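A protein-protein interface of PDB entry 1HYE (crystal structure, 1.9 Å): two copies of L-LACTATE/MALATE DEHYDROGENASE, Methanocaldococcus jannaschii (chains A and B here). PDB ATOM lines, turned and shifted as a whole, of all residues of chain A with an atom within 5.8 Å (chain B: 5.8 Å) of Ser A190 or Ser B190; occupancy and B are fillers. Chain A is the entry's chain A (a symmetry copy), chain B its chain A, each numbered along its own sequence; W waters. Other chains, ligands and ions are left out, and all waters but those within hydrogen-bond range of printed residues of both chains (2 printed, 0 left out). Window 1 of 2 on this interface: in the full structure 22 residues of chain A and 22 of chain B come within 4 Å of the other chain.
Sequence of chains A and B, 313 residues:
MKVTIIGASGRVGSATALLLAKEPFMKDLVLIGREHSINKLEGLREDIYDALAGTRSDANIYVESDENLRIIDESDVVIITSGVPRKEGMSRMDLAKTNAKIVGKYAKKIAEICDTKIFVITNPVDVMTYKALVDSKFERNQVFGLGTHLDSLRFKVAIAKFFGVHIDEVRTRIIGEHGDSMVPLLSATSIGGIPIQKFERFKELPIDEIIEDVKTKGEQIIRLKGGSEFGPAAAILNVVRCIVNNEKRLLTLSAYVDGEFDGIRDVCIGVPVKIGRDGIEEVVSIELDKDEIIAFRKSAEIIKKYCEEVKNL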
ATOM      1  N   GLU A 169       0.864  12.648 -13.038  1.00  0.00           N
ATOM      2  CA  GLU A 169       2.008  11.771 -12.822  1.00  0.00           C
ATOM      3  C   GLU A 169       1.765  10.672 -11.788  1.00  0.00           C
ATOM      4  O   GLU A 169       2.585   9.768 -11.635  1.00  0.00           O
ATOM      5  CB  GLU A 169       3.220  12.605 -12.402  1.00  0.00           C
ATOM      6  CG  GLU A 169       3.653  13.621 -13.466  1.00  0.00           C
ATOM      7  CD  GLU A 169       4.359  12.982 -14.647  1.00  0.00           C
ATOM      8  OE1 GLU A 169       4.196  11.758 -14.864  1.00  0.00           O
ATOM      9  OE2 GLU A 169       5.070  13.702 -15.374  1.00  0.00           O
ATOM     10  N   VAL A 170       0.642  10.755 -11.077  1.00  0.00           N
ATOM     11  CA  VAL A 170       0.337   9.763 -10.057  1.00  0.00           C
ATOM     12  C   VAL A 170      -0.767   8.795 -10.465  1.00  0.00           C
ATOM     13  O   VAL A 170      -1.841   9.202 -10.919  1.00  0.00           O
ATOM     14  CB  VAL A 170      -0.084  10.435  -8.722  1.00  0.00           C
ATOM     15  CG1 VAL A 170      -0.356   9.376  -7.666  1.00  0.00           C
ATOM     16  CG2 VAL A 170       1.007  11.387  -8.251  1.00  0.00           C
ATOM     17  N   ARG A 171      -0.482   7.506 -10.318  1.00  0.00           N
ATOM     18  CA  ARG A 171      -1.467   6.472 -10.612  1.00  0.00           C
ATOM     19  C   ARG A 171      -1.420   5.539  -9.413  1.00  0.00           C
ATOM     20  O   ARG A 171      -0.372   4.958  -9.096  1.00  0.00           O
ATOM     21  CB  ARG A 171      -1.119   5.725 -11.902  1.00  0.00           C
ATOM     22  CG  ARG A 171      -2.212   4.758 -12.368  1.00  0.00           C
ATOM     23  CD  ARG A 171      -3.582   5.441 -12.456  1.00  0.00           C
ATOM     24  NE  ARG A 171      -4.618   4.583 -13.042  1.00  0.00           N
ATOM     25  CZ  ARG A 171      -5.536   3.910 -12.346  1.00  0.00           C
ATOM     26  NH1 ARG A 171      -6.426   3.161 -12.986  1.00  0.00           N
ATOM     27  NH2 ARG A 171      -5.575   3.981 -11.022  1.00  0.00           N
ATOM     28  N   THR A 172      -2.554   5.407  -8.732  1.00  0.00           N
ATOM     29  CA  THR A 172      -2.619   4.556  -7.552  1.00  0.00           C
ATOM     30  C   THR A 172      -4.030   3.975  -7.434  1.00  0.00           C
ATOM     31  O   THR A 172      -4.893   4.225  -8.282  1.00  0.00           O
ATOM     32  CB  THR A 172      -2.302   5.375  -6.279  1.00  0.00           C
ATOM     33  OG1 THR A 172      -2.273   4.511  -5.136  1.00  0.00           O
ATOM     34  CG2 THR A 172      -3.370   6.452  -6.060  1.00  0.00           C
ATOM     35  N   ALA A 188       1.290  -0.973  -6.104  1.00  0.00           N
ATOM     36  CA  ALA A 188       0.762  -0.628  -7.419  1.00  0.00           C
ATOM     37  C   ALA A 188       0.548   0.885  -7.485  1.00  0.00           C
ATOM     38  O   ALA A 188      -0.464   1.362  -7.983  1.00  0.00           O
ATOM     39  CB  ALA A 188      -0.565  -1.364  -7.669  1.00  0.00           C
ATOM     40  N   THR A 189       1.516   1.626  -6.961  1.00  0.00           N
ATOM     41  CA  THR A 189       1.464   3.077  -6.953  1.00  0.00           C
ATOM     42  C   THR A 189       2.728   3.593  -7.625  1.00  0.00           C
ATOM     43  O   THR A 189       3.849   3.300  -7.184  1.00  0.00           O
ATOM     44  CB  THR A 189       1.392   3.625  -5.521  1.00  0.00           C
ATOM     45  OG1 THR A 189       0.145   3.222  -4.919  1.00  0.00           O
ATOM     46  CG2 THR A 189       1.469   5.150  -5.524  1.00  0.00           C
ATOM     47  N   SER A 190       2.544   4.347  -8.702  1.00  0.00           N
ATOM     48  CA  SER A 190       3.678   4.891  -9.423  1.00  0.00           C
ATOM     49  C   SER A 190       3.613   6.403  -9.518  1.00  0.00           C
ATOM     50  O   SER A 190       2.529   6.993  -9.496  1.00  0.00           O
ATOM     51  CB  SER A 190       3.753   4.288 -10.838  1.00  0.00           C
ATOM     52  OG  SER A 190       2.562   4.528 -11.577  1.00  0.00           O
ATOM     53  N   ILE A 191       4.791   7.017  -9.603  1.00  0.00           N
ATOM     54  CA  ILE A 191       4.930   8.467  -9.740  1.00  0.00           C
ATOM     55  C   ILE A 191       5.754   8.616 -11.017  1.00  0.00           C
ATOM     56  O   ILE A 191       6.933   8.246 -11.049  1.00  0.00           O
ATOM     57  CB  ILE A 191       5.725   9.083  -8.569  1.00  0.00           C
ATOM     58  CG1 ILE A 191       5.153   8.608  -7.228  1.00  0.00           C
ATOM     59  CG2 ILE A 191       5.678  10.614  -8.663  1.00  0.00           C
ATOM     60  CD1 ILE A 191       3.756   9.078  -6.943  1.00  0.00           C
ATOM     61  N   GLY A 192       5.144   9.133 -12.079  1.00  0.00           N
ATOM     62  CA  GLY A 192       5.861   9.261 -13.332  1.00  0.00           C
ATOM     63  C   GLY A 192       6.256   7.881 -13.849  1.00  0.00           C
ATOM     64  O   GLY A 192       7.210   7.737 -14.610  1.00  0.00           O
ATOM     65  N   GLY A 193       5.502   6.864 -13.426  1.00  0.00           N
ATOM     66  CA  GLY A 193       5.780   5.500 -13.851  1.00  0.00           C
ATOM     67  C   GLY A 193       6.749   4.775 -12.935  1.00  0.00           C
ATOM     68  O   GLY A 193       6.894   3.564 -13.011  1.00  0.00           O
ATOM     69  N   ILE A 194       7.415   5.527 -12.066  1.00  0.00           N
ATOM     70  CA  ILE A 194       8.392   4.969 -11.143  1.00  0.00           C
ATOM     71  C   ILE A 194       7.704   4.462  -9.878  1.00  0.00           C
ATOM     72  O   ILE A 194       6.862   5.152  -9.315  1.00  0.00           O
ATOM     73  CB  ILE A 194       9.428   6.047 -10.730  1.00  0.00           C
ATOM     74  CG1 ILE A 194      10.050   6.680 -11.979  1.00  0.00           C
ATOM     75  CG2 ILE A 194      10.496   5.432  -9.830  1.00  0.00           C
ATOM     76  CD1 ILE A 194      10.747   8.004 -11.705  1.00  0.00           C
ATOM     77  N   PRO A 195       8.059   3.252  -9.413  1.00  0.00           N
ATOM     78  CA  PRO A 195       7.443   2.709  -8.197  1.00  0.00           C
ATOM     79  C   PRO A 195       7.641   3.700  -7.050  1.00  0.00           C
ATOM     80  O   PRO A 195       8.748   4.206  -6.848  1.00  0.00           O
ATOM     81  CB  PRO A 195       8.204   1.408  -7.978  1.00  0.00           C
ATOM     82  CG  PRO A 195       8.554   0.980  -9.382  1.00  0.00           C
ATOM     83  CD  PRO A 195       9.003   2.286 -10.004  1.00  0.00           C
ATOM     84  N   ILE A 196       6.584   3.973  -6.294  1.00  0.00           N
ATOM     85  CA  ILE A 196       6.679   4.942  -5.207  1.00  0.00           C
ATOM     86  C   ILE A 196       7.717   4.544  -4.163  1.00  0.00           C
ATOM     87  O   ILE A 196       8.271   5.397  -3.469  1.00  0.00           O
ATOM     88  CB  ILE A 196       5.299   5.160  -4.526  1.00  0.00           C
ATOM     89  CG1 ILE A 196       5.388   6.324  -3.537  1.00  0.00           C
ATOM     90  CG2 ILE A 196       4.842   3.885  -3.835  1.00  0.00           C
ATOM     91  CD1 ILE A 196       4.057   6.739  -2.944  1.00  0.00           C
ATOM     92  N   GLU B 169      -3.448   4.945 -19.194  1.00  0.00           N
ATOM     93  CA  GLU B 169      -3.022   3.973 -18.195  1.00  0.00           C
ATOM     94  C   GLU B 169      -1.539   3.611 -18.271  1.00  0.00           C
ATOM     95  O   GLU B 169      -1.016   2.934 -17.386  1.00  0.00           O
ATOM     96  CB  GLU B 169      -3.862   2.701 -18.328  1.00  0.00           C
ATOM     97  CG  GLU B 169      -5.358   2.937 -18.085  1.00  0.00           C
ATOM     98  CD  GLU B 169      -5.698   3.145 -16.622  1.00  0.00           C
ATOM     99  OE1 GLU B 169      -4.791   3.493 -15.829  1.00  0.00           O
ATOM    100  OE2 GLU B 169      -6.878   2.977 -16.257  1.00  0.00           O
ATOM    101  N   VAL B 170      -0.865   4.058 -19.329  1.00  0.00           N
ATOM    102  CA  VAL B 170       0.547   3.746 -19.493  1.00  0.00           C
ATOM    103  C   VAL B 170       1.463   4.935 -19.231  1.00  0.00           C
ATOM    104  O   VAL B 170       1.262   6.031 -19.763  1.00  0.00           O
ATOM    105  CB  VAL B 170       0.847   3.216 -20.921  1.00  0.00           C
ATOM    106  CG1 VAL B 170       2.320   2.862 -21.050  1.00  0.00           C
ATOM    107  CG2 VAL B 170      -0.020   2.001 -21.220  1.00  0.00           C
ATOM    108  N   ARG B 171       2.463   4.711 -18.384  1.00  0.00           N
ATOM    109  CA  ARG B 171       3.451   5.741 -18.087  1.00  0.00           C
ATOM    110  C   ARG B 171       4.793   5.039 -18.213  1.00  0.00           C
ATOM    111  O   ARG B 171       5.070   4.059 -17.505  1.00  0.00           O
ATOM    112  CB  ARG B 171       3.258   6.307 -16.678  1.00  0.00           C
ATOM    113  CG  ARG B 171       4.140   7.521 -16.375  1.00  0.00           C
ATOM    114  CD  ARG B 171       4.007   8.608 -17.449  1.00  0.00           C
ATOM    115  NE  ARG B 171       4.723   9.843 -17.111  1.00  0.00           N
ATOM    116  CZ  ARG B 171       5.917  10.191 -17.593  1.00  0.00           C
ATOM    117  NH1 ARG B 171       6.470  11.336 -17.213  1.00  0.00           N
ATOM    118  NH2 ARG B 171       6.560   9.409 -18.450  1.00  0.00           N
ATOM    119  N   THR B 172       5.624   5.527 -19.127  1.00  0.00           N
ATOM    120  CA  THR B 172       6.928   4.919 -19.350  1.00  0.00           C
ATOM    121  C   THR B 172       7.914   6.001 -19.797  1.00  0.00           C
ATOM    122  O   THR B 172       7.562   7.182 -19.888  1.00  0.00           O
ATOM    123  CB  THR B 172       6.837   3.834 -20.449  1.00  0.00           C
ATOM    124  OG1 THR B 172       8.102   3.174 -20.591  1.00  0.00           O
ATOM    125  CG2 THR B 172       6.453   4.467 -21.790  1.00  0.00           C
ATOM    126  N   ALA B 188      10.753   1.341 -14.820  1.00  0.00           N
ATOM    127  CA  ALA B 188       9.974   2.535 -14.515  1.00  0.00           C
ATOM    128  C   ALA B 188       8.815   2.638 -15.509  1.00  0.00           C
ATOM    129  O   ALA B 188       8.515   3.706 -16.026  1.00  0.00           O
ATOM    130  CB  ALA B 188      10.862   3.788 -14.603  1.00  0.00           C
ATOM    131  N   THR B 189       8.183   1.502 -15.774  1.00  0.00           N
ATOM    132  CA  THR B 189       7.059   1.435 -16.691  1.00  0.00           C
ATOM    133  C   THR B 189       5.887   0.812 -15.948  1.00  0.00           C
ATOM    134  O   THR B 189       5.976  -0.321 -15.453  1.00  0.00           O
ATOM    135  CB  THR B 189       7.392   0.579 -17.921  1.00  0.00           C
ATOM    136  OG1 THR B 189       8.434   1.225 -18.682  1.00  0.00           O
ATOM    137  CG2 THR B 189       6.162   0.414 -18.810  1.00  0.00           C
ATOM    138  N   SER B 190       4.795   1.560 -15.857  1.00  0.00           N
ATOM    139  CA  SER B 190       3.618   1.066 -15.170  1.00  0.00           C
ATOM    140  C   SER B 190       2.397   1.070 -16.069  1.00  0.00           C
ATOM    141  O   SER B 190       2.300   1.870 -17.005  1.00  0.00           O
ATOM    142  CB  SER B 190       3.336   1.914 -13.916  1.00  0.00           C
ATOM    143  OG  SER B 190       3.156   3.288 -14.236  1.00  0.00           O
ATOM    144  N   ILE B 191       1.479   0.148 -15.783  1.00  0.00           N
ATOM    145  CA  ILE B 191       0.219   0.020 -16.513  1.00  0.00           C
ATOM    146  C   ILE B 191      -0.833   0.138 -15.411  1.00  0.00           C
ATOM    147  O   ILE B 191      -0.946  -0.746 -14.556  1.00  0.00           O
ATOM    148  CB  ILE B 191       0.077  -1.365 -17.179  1.00  0.00           C
ATOM    149  CG1 ILE B 191       1.335  -1.699 -17.989  1.00  0.00           C
ATOM    150  CG2 ILE B 191      -1.164  -1.380 -18.081  1.00  0.00           C
ATOM    151  CD1 ILE B 191       1.573  -0.804 -19.170  1.00  0.00           C
ATOM    152  N   GLY B 192      -1.589   1.231 -15.406  1.00  0.00           N
ATOM    153  CA  GLY B 192      -2.576   1.421 -14.362  1.00  0.00           C
ATOM    154  C   GLY B 192      -1.885   1.522 -13.006  1.00  0.00           C
ATOM    155  O   GLY B 192      -2.481   1.243 -11.967  1.00  0.00           O
ATOM    156  N   GLY B 193      -0.614   1.930 -13.029  1.00  0.00           N
ATOM    157  CA  GLY B 193       0.150   2.067 -11.798  1.00  0.00           C
ATOM    158  C   GLY B 193       0.877   0.794 -11.403  1.00  0.00           C
ATOM    159  O   GLY B 193       1.745   0.812 -10.544  1.00  0.00           O
ATOM    160  N   ILE B 194       0.514  -0.315 -12.038  1.00  0.00           N
ATOM    161  CA  ILE B 194       1.110  -1.609 -11.744  1.00  0.00           C
ATOM    162  C   ILE B 194       2.393  -1.802 -12.550  1.00  0.00           C
ATOM    163  O   ILE B 194       2.418  -1.530 -13.744  1.00  0.00           O
ATOM    164  CB  ILE B 194       0.132  -2.755 -12.113  1.00  0.00           C
ATOM    165  CG1 ILE B 194      -1.220  -2.528 -11.428  1.00  0.00           C
ATOM    166  CG2 ILE B 194       0.731  -4.103 -11.724  1.00  0.00           C
ATOM    167  CD1 ILE B 194      -2.354  -3.339 -12.039  1.00  0.00           C
ATOM    168  N   PRO B 195       3.472  -2.281 -11.906  1.00  0.00           N
ATOM    169  CA  PRO B 195       4.733  -2.498 -12.623  1.00  0.00           C
ATOM    170  C   PRO B 195       4.479  -3.424 -13.813  1.00  0.00           C
ATOM    171  O   PRO B 195       3.820  -4.457 -13.669  1.00  0.00           O
ATOM    172  CB  PRO B 195       5.622  -3.141 -11.566  1.00  0.00           C
ATOM    173  CG  PRO B 195       5.117  -2.530 -10.282  1.00  0.00           C
ATOM    174  CD  PRO B 195       3.616  -2.597 -10.474  1.00  0.00           C
ATOM    175  N   ILE B 196       5.004  -3.071 -14.980  1.00  0.00           N
ATOM    176  CA  ILE B 196       4.772  -3.877 -16.174  1.00  0.00           C
ATOM    177  C   ILE B 196       5.284  -5.305 -16.019  1.00  0.00           C
ATOM    178  O   ILE B 196       4.788  -6.226 -16.669  1.00  0.00           O
ATOM    179  CB  ILE B 196       5.407  -3.219 -17.430  1.00  0.00           C
ATOM    180  CG1 ILE B 196       4.972  -3.975 -18.686  1.00  0.00           C
ATOM    181  CG2 ILE B 196       6.923  -3.190 -17.303  1.00  0.00           C
ATOM    182  CD1 ILE B 196       5.392  -3.316 -19.985  1.00  0.00           C
HETATM  183  O   HOH W   1      -2.687   1.131  -9.285  1.00  0.00           O
HETATM  184  O   HOH W   2       8.756   6.272 -16.256  1.00  0.00           O
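The backbone carbonyl oxygen (O) of Glu A169 sits at hydrogen-bond distance from the backbone NH (N) of Gly A192, 2.7 Å away.
The backbone carbonyl oxygen of Thr A189 sits at hydrogen-bond distance from the backbone NH of Ile A196 (3.0 Å).
The backbone carbonyl oxygen (O) of Arg B171 lies within hydrogen-bond range of the backbone NH (N) of Ser B190 (3.0 Å).
N of Gly B192 lies within hydrogen-bond range of O of Glu B169.
The side-chain hydroxyl (OG1) of Thr B172 lies within hydrogen-bond range of the side-chain hydroxyl (OG1) of Thr B189, 2.7 Å away.
The side-chain hydroxyl (OG1) of Thr A172 is in hydrogen-bond range of the side-chain hydroxyl (OG1) of Thr A189.
O of Ala A188 sits close to O of Gly B193 (3.4 Å).
O of Gly A193 lies close to O of Ala B188.
The side-chain hydroxyl (OG) of Ser B190 is in hydrogen-bond range of the side-chain hydroxyl (OG) of Ser A190 (3.0 Å).
NE of Arg B171 is in salt-bridge range of OE1 of Glu A169, 3.0 Å away.
The side-chain carboxylate (OE1) of Glu B169 lies within salt-bridge range of the guanidinium group (NE) of Arg A171 (3.0 Å).
Water W2 bridges the backbone carbonyl oxygen of Ala B188 and the backbone carbonyl oxygen of Gly A192.
Water W1 bridges the backbone carbonyl oxygen (O) of Ala A188 (2.6 Å) and the backbone carbonyl oxygen (O) of Gly B192 (2.7 Å).
Among the printed residues, pairs that only touch across the chains: Arg A171 with Gly B192 (3.3 Å), Arg A171 with Gly B193 (3.3 Å), Ala A188 with Ile B194 (3.99 Å), Thr A189 with Gly B193 (3.7 Å), Ser A190 with Gly B193 (3.5 Å), Gly A192 with Arg B171 (3.3 Å), Gly A193 with Arg B171 (3.3 Å), Gly A193 with Thr B189 (3.7 Å), Gly A193 with Ser B190 (3.5 Å) and Ile A194 with Ala B188 (3.99 Å).
Printed residues of chain B that touch a printed residue of chain A: Glu B169, Arg B171, Ala B188, Thr B189, Ser B190, Gly B192, Gly B193 and Ile B194.
Of the 13 printed residues of chain A, 8 touch a printed residue of chain B.
Printed residues of chain A that touch a printed residue of chain B: Glu A169, Arg A171, Ala A188, Thr A189, Ser A190, Gly A192, Gly A193 and Ile A194.
Hydrophobic or aromatic side chains of chain A within 4 Å of the printed part of chain B: Ala A188 and Ile A194.
Among the printed residues, 15 pairs touch across the chains.
Among the printed residues, Asp or Glu carboxylates within 4 Å of a Lys or Arg side-chain nitrogen of the other chain: Glu A169 with Arg B171 (3.0 Å) and Arg A171 with Glu B169 (3.0 Å).
Ala A188 touches Gly B193, and with the chains exchanged Gly A193 touches Ala B188.
Ala A188 touches Ile B194, and with the chains exchanged Ile A194 touches Ala B188.
Thr A189 touches Gly B193, and with the chains exchanged Gly A193 touches Thr B189.
Ser A190 touches its own counterpart, Ser B190.
13 positions are printed for both chains.
Of the 15 pairs that touch across the chains among the printed residues, 15 have their exchanged pair printed and touching as well.
Of chain B, only Ser B190 and Gly B193 come within 4 Å of Ser A190.
Ser B190 touches just these residues of chain A: Ser A190 and Gly A193.
Of the printed residues of chain A, Ala B188 touches Gly A193 (3.3 Å) and Ile A194 (3.99 Å).
Of the printed residues of chain B, Gly A192 touches Arg B171.
Of the printed residues of chain B, Ala A188 touches Gly B193 and Ile B194.
Of the printed residues of chain A, Thr B189 touches Gly A193.
Of the printed residues of chain A, Gly B192 touches Arg A171.
The nearest residue of chain B that does not touch Ser A190 is Ile B194 (5.3 Å).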
